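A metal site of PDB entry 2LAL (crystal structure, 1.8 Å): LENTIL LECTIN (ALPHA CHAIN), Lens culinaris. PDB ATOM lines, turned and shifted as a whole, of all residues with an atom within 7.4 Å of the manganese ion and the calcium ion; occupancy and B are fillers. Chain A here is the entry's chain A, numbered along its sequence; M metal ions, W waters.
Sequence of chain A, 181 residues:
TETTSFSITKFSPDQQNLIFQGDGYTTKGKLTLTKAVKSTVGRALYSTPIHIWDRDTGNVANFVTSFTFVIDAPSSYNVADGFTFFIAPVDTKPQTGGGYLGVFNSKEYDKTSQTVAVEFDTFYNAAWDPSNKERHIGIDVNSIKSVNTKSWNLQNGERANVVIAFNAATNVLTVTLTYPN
Water W1 bridges OE1 of Glu 119 (2.7 Å) and O of Ile 144 (2.8 Å).
Water W3 lies within hydrogen-bond range of the backbone carbonyl oxygen of Gly 99 (2.7 Å) and the indole nitrogen of Trp 128 (3.1 Å).
The backbone carbonyl oxygen of Glu 134 sits at hydrogen-bond distance from a ring nitrogen (ND1) of His 136, at 2.9 Å.
The side-chain hydroxyl (OG) of Ser 146 lies close to the side-chain carboxylate (OE2) of Glu 119 (3.4 Å).
OE1 of Glu 119 sits close to OD2 of Asp 140 (2.6 Å).
N of Gly 138 is in hydrogen-bond range of O of Glu 119, 2.9 Å away.
Of the 26 residues printed, 4 come within 4 Å of the calcium ion.
The nearest printed residue that does not touch the calcium ion is Trp 128 (4.4 Å).
Four residues have an atom within 4 Å of the manganese ion: Glu 119, Asp 121, Asp 129 and His 136.
The manganese ion is bound by water W2 (2.2 Å), water W1 (2.2 Å), the side-chain carboxylate of Asp 129 (2.4 Å), a ring nitrogen (NE2) of His 136 (2.4 Å), the side-chain carboxylate of Glu 119 (2.4 Å) and the side-chain carboxylate of Asp 121 (2.4 Å).
The manganese ion has six donor atoms within binding distance.
The calcium ion is bound by the side-chain carboxylate (OD2) of Asp 121, the backbone carbonyl oxygen (O) of Phe 123, the side-chain amide oxygen (OD1) of Asn 125, the side-chain carboxylate (OD1) of Asp 121, the side-chain carboxylate (OD2) of Asp 129, water W3 and water W4.
The calcium ion has seven donor atoms within binding distance.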
ATOM      1  N   ASP A  81      20.146  14.061 -18.014  1.00  0.00           N
ATOM      2  CA  ASP A  81      19.953  14.026 -16.559  1.00  0.00           C
ATOM      3  C   ASP A  81      19.449  15.371 -16.050  1.00  0.00           C
ATOM      4  O   ASP A  81      18.788  15.490 -15.019  1.00  0.00           O
ATOM      5  CB  ASP A  81      21.277  13.683 -15.871  1.00  0.00           C
ATOM      6  CG  ASP A  81      21.338  12.172 -15.580  1.00  0.00           C
ATOM      7  OD1 ASP A  81      20.625  11.751 -14.668  1.00  0.00           O
ATOM      8  OD2 ASP A  81      21.999  11.444 -16.302  1.00  0.00           O
ATOM      9  N   GLY A  82      19.884  16.407 -16.763  1.00  0.00           N
ATOM     10  CA  GLY A  82      19.403  17.758 -16.465  1.00  0.00           C
ATOM     11  C   GLY A  82      20.565  18.788 -16.549  1.00  0.00           C
ATOM     12  O   GLY A  82      21.601  18.478 -17.053  1.00  0.00           O
ATOM     13  N   GLY A  98      26.300  12.066 -14.829  1.00  0.00           N
ATOM     14  CA  GLY A  98      25.048  11.262 -14.629  1.00  0.00           C
ATOM     15  C   GLY A  98      24.194  12.013 -13.631  1.00  0.00           C
ATOM     16  O   GLY A  98      24.129  13.224 -13.787  1.00  0.00           O
ATOM     17  N   GLY A  99      23.493  11.423 -12.692  1.00  0.00           N
ATOM     18  CA  GLY A  99      22.494  12.220 -11.969  1.00  0.00           C
ATOM     19  C   GLY A  99      23.244  13.137 -10.993  1.00  0.00           C
ATOM     20  O   GLY A  99      22.526  13.861 -10.279  1.00  0.00           O
ATOM     21  N   TYR A 100      24.569  13.096 -10.860  1.00  0.00           N
ATOM     22  CA  TYR A 100      25.248  14.088  -9.980  1.00  0.00           C
ATOM     23  C   TYR A 100      25.515  15.377 -10.765  1.00  0.00           C
ATOM     24  O   TYR A 100      26.038  16.278 -10.122  1.00  0.00           O
ATOM     25  CB  TYR A 100      26.567  13.564  -9.446  1.00  0.00           C
ATOM     26  CG  TYR A 100      26.406  12.503  -8.350  1.00  0.00           C
ATOM     27  CD1 TYR A 100      26.091  12.746  -7.026  1.00  0.00           C
ATOM     28  CD2 TYR A 100      26.591  11.184  -8.760  1.00  0.00           C
ATOM     29  CE1 TYR A 100      25.946  11.697  -6.101  1.00  0.00           C
ATOM     30  CE2 TYR A 100      26.471  10.165  -7.854  1.00  0.00           C
ATOM     31  CZ  TYR A 100      26.136  10.400  -6.530  1.00  0.00           C
ATOM     32  OH  TYR A 100      26.049   9.272  -5.738  1.00  0.00           O
ATOM     33  N   LEU A 101      25.173  15.442 -12.005  1.00  0.00           N
ATOM     34  CA  LEU A 101      25.051  16.579 -12.911  1.00  0.00           C
ATOM     35  C   LEU A 101      26.417  17.257 -13.126  1.00  0.00           C
ATOM     36  O   LEU A 101      26.340  18.450 -13.513  1.00  0.00           O
ATOM     37  CB  LEU A 101      24.030  17.592 -12.434  1.00  0.00           C
ATOM     38  CG  LEU A 101      22.617  17.220 -12.412  1.00  0.00           C
ATOM     39  CD1 LEU A 101      21.680  18.083 -11.590  1.00  0.00           C
ATOM     40  CD2 LEU A 101      21.929  16.738 -13.662  1.00  0.00           C
ATOM     41  N   GLU A 119      19.267  23.279  -9.827  1.00  0.00           N
ATOM     42  CA  GLU A 119      19.174  22.266 -10.874  1.00  0.00           C
ATOM     43  C   GLU A 119      17.747  22.274 -11.464  1.00  0.00           C
ATOM     44  O   GLU A 119      16.787  22.665 -10.840  1.00  0.00           O
ATOM     45  CB  GLU A 119      19.474  20.879 -10.337  1.00  0.00           C
ATOM     46  CG  GLU A 119      18.560  20.715  -9.104  1.00  0.00           C
ATOM     47  CD  GLU A 119      18.590  19.338  -8.570  1.00  0.00           C
ATOM     48  OE1 GLU A 119      19.607  18.784  -8.258  1.00  0.00           O
ATOM     49  OE2 GLU A 119      17.600  18.597  -8.506  1.00  0.00           O
ATOM     50  N   PHE A 120      17.738  21.916 -12.701  1.00  0.00           N
ATOM     51  CA  PHE A 120      16.552  21.619 -13.545  1.00  0.00           C
ATOM     52  C   PHE A 120      16.643  20.144 -13.914  1.00  0.00           C
ATOM     53  O   PHE A 120      17.537  19.757 -14.596  1.00  0.00           O
ATOM     54  CB  PHE A 120      16.658  22.488 -14.812  1.00  0.00           C
ATOM     55  CG  PHE A 120      16.706  23.963 -14.316  1.00  0.00           C
ATOM     56  CD1 PHE A 120      15.566  24.681 -14.032  1.00  0.00           C
ATOM     57  CD2 PHE A 120      17.960  24.568 -14.120  1.00  0.00           C
ATOM     58  CE1 PHE A 120      15.595  25.999 -13.568  1.00  0.00           C
ATOM     59  CE2 PHE A 120      18.047  25.876 -13.658  1.00  0.00           C
ATOM     60  CZ  PHE A 120      16.900  26.586 -13.373  1.00  0.00           C
ATOM     61  N   ASP A 121      16.048  19.341 -13.012  1.00  0.00           N
ATOM     62  CA  ASP A 121      16.513  17.926 -12.990  1.00  0.00           C
ATOM     63  C   ASP A 121      15.467  17.069 -13.728  1.00  0.00           C
ATOM     64  O   ASP A 121      14.292  17.208 -13.312  1.00  0.00           O
ATOM     65  CB  ASP A 121      16.585  17.434 -11.541  1.00  0.00           C
ATOM     66  CG  ASP A 121      17.006  15.978 -11.409  1.00  0.00           C
ATOM     67  OD1 ASP A 121      17.116  15.161 -12.337  1.00  0.00           O
ATOM     68  OD2 ASP A 121      17.401  15.508 -10.308  1.00  0.00           O
ATOM     69  N   THR A 122      15.766  16.338 -14.770  1.00  0.00           N
ATOM     70  CA  THR A 122      14.832  15.741 -15.715  1.00  0.00           C
ATOM     71  C   THR A 122      14.705  14.233 -15.519  1.00  0.00           C
ATOM     72  O   THR A 122      13.928  13.579 -16.290  1.00  0.00           O
ATOM     73  CB  THR A 122      15.248  16.046 -17.142  1.00  0.00           C
ATOM     74  OG1 THR A 122      16.550  15.571 -17.397  1.00  0.00           O
ATOM     75  CG2 THR A 122      15.134  17.511 -17.412  1.00  0.00           C
ATOM     76  N   PHE A 123      15.318  13.610 -14.577  1.00  0.00           N
ATOM     77  CA  PHE A 123      15.479  12.184 -14.317  1.00  0.00           C
ATOM     78  C   PHE A 123      15.449  11.833 -12.862  1.00  0.00           C
ATOM     79  O   PHE A 123      16.219  12.387 -12.073  1.00  0.00           O
ATOM     80  CB  PHE A 123      16.702  11.642 -15.021  1.00  0.00           C
ATOM     81  CG  PHE A 123      16.733  10.128 -15.060  1.00  0.00           C
ATOM     82  CD1 PHE A 123      16.063   9.487 -16.064  1.00  0.00           C
ATOM     83  CD2 PHE A 123      17.475   9.513 -14.051  1.00  0.00           C
ATOM     84  CE1 PHE A 123      16.177   8.140 -16.031  1.00  0.00           C
ATOM     85  CE2 PHE A 123      17.549   8.121 -14.028  1.00  0.00           C
ATOM     86  CZ  PHE A 123      16.879   7.466 -15.072  1.00  0.00           C
ATOM     87  N   TYR A 124      14.473  11.029 -12.420  1.00  0.00           N
ATOM     88  CA  TYR A 124      14.303  10.522 -11.043  1.00  0.00           C
ATOM     89  C   TYR A 124      15.401   9.525 -10.692  1.00  0.00           C
ATOM     90  O   TYR A 124      15.508   8.394 -11.176  1.00  0.00           O
ATOM     91  CB  TYR A 124      12.951   9.804 -10.929  1.00  0.00           C
ATOM     92  CG  TYR A 124      12.715   9.235  -9.522  1.00  0.00           C
ATOM     93  CD1 TYR A 124      12.611  10.050  -8.404  1.00  0.00           C
ATOM     94  CD2 TYR A 124      12.566   7.840  -9.343  1.00  0.00           C
ATOM     95  CE1 TYR A 124      12.389   9.534  -7.146  1.00  0.00           C
ATOM     96  CE2 TYR A 124      12.353   7.303  -8.076  1.00  0.00           C
ATOM     97  CZ  TYR A 124      12.261   8.147  -6.968  1.00  0.00           C
ATOM     98  OH  TYR A 124      12.030   7.652  -5.700  1.00  0.00           O
ATOM     99  N   ASN A 125      16.283   9.928  -9.798  1.00  0.00           N
ATOM    100  CA  ASN A 125      17.260   9.080  -9.110  1.00  0.00           C
ATOM    101  C   ASN A 125      16.704   8.710  -7.731  1.00  0.00           C
ATOM    102  O   ASN A 125      16.451   9.599  -6.977  1.00  0.00           O
ATOM    103  CB  ASN A 125      18.590   9.818  -8.923  1.00  0.00           C
ATOM    104  CG  ASN A 125      19.086  10.227 -10.310  1.00  0.00           C
ATOM    105  OD1 ASN A 125      18.827  11.432 -10.812  1.00  0.00           O
ATOM    106  ND2 ASN A 125      19.760   9.315 -11.006  1.00  0.00           N
ATOM    107  N   ALA A 126      16.339   7.464  -7.613  1.00  0.00           N
ATOM    108  CA  ALA A 126      15.494   6.960  -6.519  1.00  0.00           C
ATOM    109  C   ALA A 126      16.136   7.231  -5.161  1.00  0.00           C
ATOM    110  O   ALA A 126      15.413   7.496  -4.195  1.00  0.00           O
ATOM    111  CB  ALA A 126      15.388   5.432  -6.694  1.00  0.00           C
ATOM    112  N   TRP A 128      17.825   9.825  -4.050  1.00  0.00           N
ATOM    113  CA  TRP A 128      17.844  11.191  -3.555  1.00  0.00           C
ATOM    114  C   TRP A 128      16.749  12.050  -4.139  1.00  0.00           C
ATOM    115  O   TRP A 128      16.422  13.057  -3.482  1.00  0.00           O
ATOM    116  CB  TRP A 128      19.201  11.838  -3.681  1.00  0.00           C
ATOM    117  CG  TRP A 128      19.697  12.007  -5.112  1.00  0.00           C
ATOM    118  CD1 TRP A 128      19.200  12.913  -6.022  1.00  0.00           C
ATOM    119  CD2 TRP A 128      20.730  11.274  -5.744  1.00  0.00           C
ATOM    120  NE1 TRP A 128      19.934  12.717  -7.227  1.00  0.00           N
ATOM    121  CE2 TRP A 128      20.818  11.760  -7.069  1.00  0.00           C
ATOM    122  CE3 TRP A 128      21.609  10.270  -5.377  1.00  0.00           C
ATOM    123  CZ2 TRP A 128      21.715  11.278  -7.913  1.00  0.00           C
ATOM    124  CZ3 TRP A 128      22.528   9.754  -6.262  1.00  0.00           C
ATOM    125  CH2 TRP A 128      22.581  10.258  -7.535  1.00  0.00           C
ATOM    126  N   ASP A 129      16.175  11.815  -5.298  1.00  0.00           N
ATOM    127  CA  ASP A 129      15.183  12.718  -5.905  1.00  0.00           C
ATOM    128  C   ASP A 129      13.848  12.599  -5.190  1.00  0.00           C
ATOM    129  O   ASP A 129      13.653  11.539  -4.583  1.00  0.00           O
ATOM    130  CB  ASP A 129      14.996  12.380  -7.387  1.00  0.00           C
ATOM    131  CG  ASP A 129      16.164  13.083  -8.096  1.00  0.00           C
ATOM    132  OD1 ASP A 129      16.643  14.088  -7.481  1.00  0.00           O
ATOM    133  OD2 ASP A 129      16.592  12.729  -9.155  1.00  0.00           O
ATOM    134  N   PRO A 130      12.997  13.634  -5.247  1.00  0.00           N
ATOM    135  CA  PRO A 130      11.673  13.546  -4.602  1.00  0.00           C
ATOM    136  C   PRO A 130      10.887  12.370  -5.172  1.00  0.00           C
ATOM    137  O   PRO A 130      10.942  12.036  -6.350  1.00  0.00           O
ATOM    138  CB  PRO A 130      11.055  14.853  -5.031  1.00  0.00           C
ATOM    139  CG  PRO A 130      12.129  15.771  -5.504  1.00  0.00           C
ATOM    140  CD  PRO A 130      13.147  14.852  -6.090  1.00  0.00           C
ATOM    141  N   GLU A 134       8.542  13.287  -9.973  1.00  0.00           N
ATOM    142  CA  GLU A 134       8.500  14.207 -11.096  1.00  0.00           C
ATOM    143  C   GLU A 134       9.767  15.011 -11.236  1.00  0.00           C
ATOM    144  O   GLU A 134      10.648  14.990 -10.410  1.00  0.00           O
ATOM    145  CB  GLU A 134       7.265  15.032 -11.167  1.00  0.00           C
ATOM    146  CG  GLU A 134       6.593  15.388  -9.931  1.00  0.00           C
ATOM    147  CD  GLU A 134       5.100  15.602 -10.076  1.00  0.00           C
ATOM    148  OE1 GLU A 134       4.430  14.709 -10.604  1.00  0.00           O
ATOM    149  OE2 GLU A 134       4.517  16.617  -9.661  1.00  0.00           O
ATOM    150  N   HIS A 136      11.926  18.499 -11.773  1.00  0.00           N
ATOM    151  CA  HIS A 136      11.809  19.498 -10.711  1.00  0.00           C
ATOM    152  C   HIS A 136      13.004  20.459 -10.766  1.00  0.00           C
ATOM    153  O   HIS A 136      14.011  20.120 -11.350  1.00  0.00           O
ATOM    154  CB  HIS A 136      11.697  18.860  -9.328  1.00  0.00           C
ATOM    155  CG  HIS A 136      12.808  17.838  -9.078  1.00  0.00           C
ATOM    156  ND1 HIS A 136      12.904  16.544  -9.604  1.00  0.00           N
ATOM    157  CD2 HIS A 136      13.948  18.069  -8.274  1.00  0.00           C
ATOM    158  CE1 HIS A 136      14.087  15.991  -9.167  1.00  0.00           C
ATOM    159  NE2 HIS A 136      14.739  16.927  -8.377  1.00  0.00           N
ATOM    160  N   ILE A 137      12.746  21.629 -10.267  1.00  0.00           N
ATOM    161  CA  ILE A 137      13.741  22.661  -9.936  1.00  0.00           C
ATOM    162  C   ILE A 137      14.277  22.413  -8.524  1.00  0.00           C
ATOM    163  O   ILE A 137      13.375  22.117  -7.724  1.00  0.00           O
ATOM    164  CB  ILE A 137      13.057  24.040  -9.982  1.00  0.00           C
ATOM    165  CG1 ILE A 137      12.446  24.261 -11.362  1.00  0.00           C
ATOM    166  CG2 ILE A 137      14.013  25.146  -9.598  1.00  0.00           C
ATOM    167  CD1 ILE A 137      11.184  25.056 -11.442  1.00  0.00           C
ATOM    168  N   GLY A 138      15.533  22.407  -8.229  1.00  0.00           N
ATOM    169  CA  GLY A 138      15.992  22.254  -6.814  1.00  0.00           C
ATOM    170  C   GLY A 138      17.049  23.311  -6.484  1.00  0.00           C
ATOM    171  O   GLY A 138      17.765  23.795  -7.385  1.00  0.00           O
ATOM    172  N   ASP A 140      20.445  23.200  -4.378  1.00  0.00           N
ATOM    173  CA  ASP A 140      21.457  22.252  -3.903  1.00  0.00           C
ATOM    174  C   ASP A 140      22.598  22.960  -3.191  1.00  0.00           C
ATOM    175  O   ASP A 140      23.239  23.844  -3.763  1.00  0.00           O
ATOM    176  CB  ASP A 140      22.013  21.441  -5.074  1.00  0.00           C
ATOM    177  CG  ASP A 140      20.907  20.730  -5.857  1.00  0.00           C
ATOM    178  OD1 ASP A 140      19.767  20.652  -5.457  1.00  0.00           O
ATOM    179  OD2 ASP A 140      21.303  20.232  -6.887  1.00  0.00           O
ATOM    180  N   ILE A 144      23.825  16.641  -3.881  1.00  0.00           N
ATOM    181  CA  ILE A 144      22.859  16.349  -4.940  1.00  0.00           C
ATOM    182  C   ILE A 144      21.441  16.223  -4.463  1.00  0.00           C
ATOM    183  O   ILE A 144      20.428  16.373  -5.143  1.00  0.00           O
ATOM    184  CB  ILE A 144      23.279  15.168  -5.784  1.00  0.00           C
ATOM    185  CG1 ILE A 144      22.653  15.189  -7.157  1.00  0.00           C
ATOM    186  CG2 ILE A 144      23.019  13.846  -5.070  1.00  0.00           C
ATOM    187  CD1 ILE A 144      22.896  16.379  -8.052  1.00  0.00           C
ATOM    188  N   LYS A 145      21.285  16.008  -3.152  1.00  0.00           N
ATOM    189  CA  LYS A 145      19.918  15.997  -2.584  1.00  0.00           C
ATOM    190  C   LYS A 145      19.474  17.435  -2.285  1.00  0.00           C
ATOM    191  O   LYS A 145      20.046  17.951  -1.311  1.00  0.00           O
ATOM    192  CB  LYS A 145      20.010  15.288  -1.209  1.00  0.00           C
ATOM    193  CG  LYS A 145      19.099  14.065  -1.256  1.00  0.00           C
ATOM    194  CD  LYS A 145      17.961  14.295  -0.280  1.00  0.00           C
ATOM    195  CE  LYS A 145      18.592  14.601   1.069  1.00  0.00           C
ATOM    196  NZ  LYS A 145      17.567  15.130   1.978  1.00  0.00           N
ATOM    197  N   SER A 146      18.564  18.027  -3.010  1.00  0.00           N
ATOM    198  CA  SER A 146      18.180  19.438  -2.913  1.00  0.00           C
ATOM    199  C   SER A 146      17.730  19.812  -1.523  1.00  0.00           C
ATOM    200  O   SER A 146      17.089  18.968  -0.861  1.00  0.00           O
ATOM    201  CB  SER A 146      17.109  19.769  -3.938  1.00  0.00           C
ATOM    202  OG  SER A 146      17.534  19.191  -5.171  1.00  0.00           O
ATOM    203  N   THR A 149      12.751  21.691  -3.473  1.00  0.00           N
ATOM    204  CA  THR A 149      12.386  21.311  -4.840  1.00  0.00           C
ATOM    205  C   THR A 149      10.995  21.834  -5.172  1.00  0.00           C
ATOM    206  O   THR A 149      10.174  22.051  -4.285  1.00  0.00           O
ATOM    207  CB  THR A 149      12.501  19.843  -5.090  1.00  0.00           C
ATOM    208  OG1 THR A 149      11.530  19.075  -4.367  1.00  0.00           O
ATOM    209  CG2 THR A 149      13.857  19.325  -4.747  1.00  0.00           C
HETATM  210 MN    MN M   1      17.021  16.330  -8.091  1.00  0.00          MN
HETATM  211 CA    CA M   2      17.862  13.455 -11.008  1.00  0.00          CA
HETATM  212  O   HOH W   1      19.161  16.217  -7.592  1.00  0.00           O
HETATM  213  O   HOH W   2      16.646  16.895  -6.049  1.00  0.00           O
HETATM  214  O   HOH W   3      19.872  14.136  -9.941  1.00  0.00           O
HETATM  215  O   HOH W   4      19.093  13.536 -13.062  1.00  0.00           O
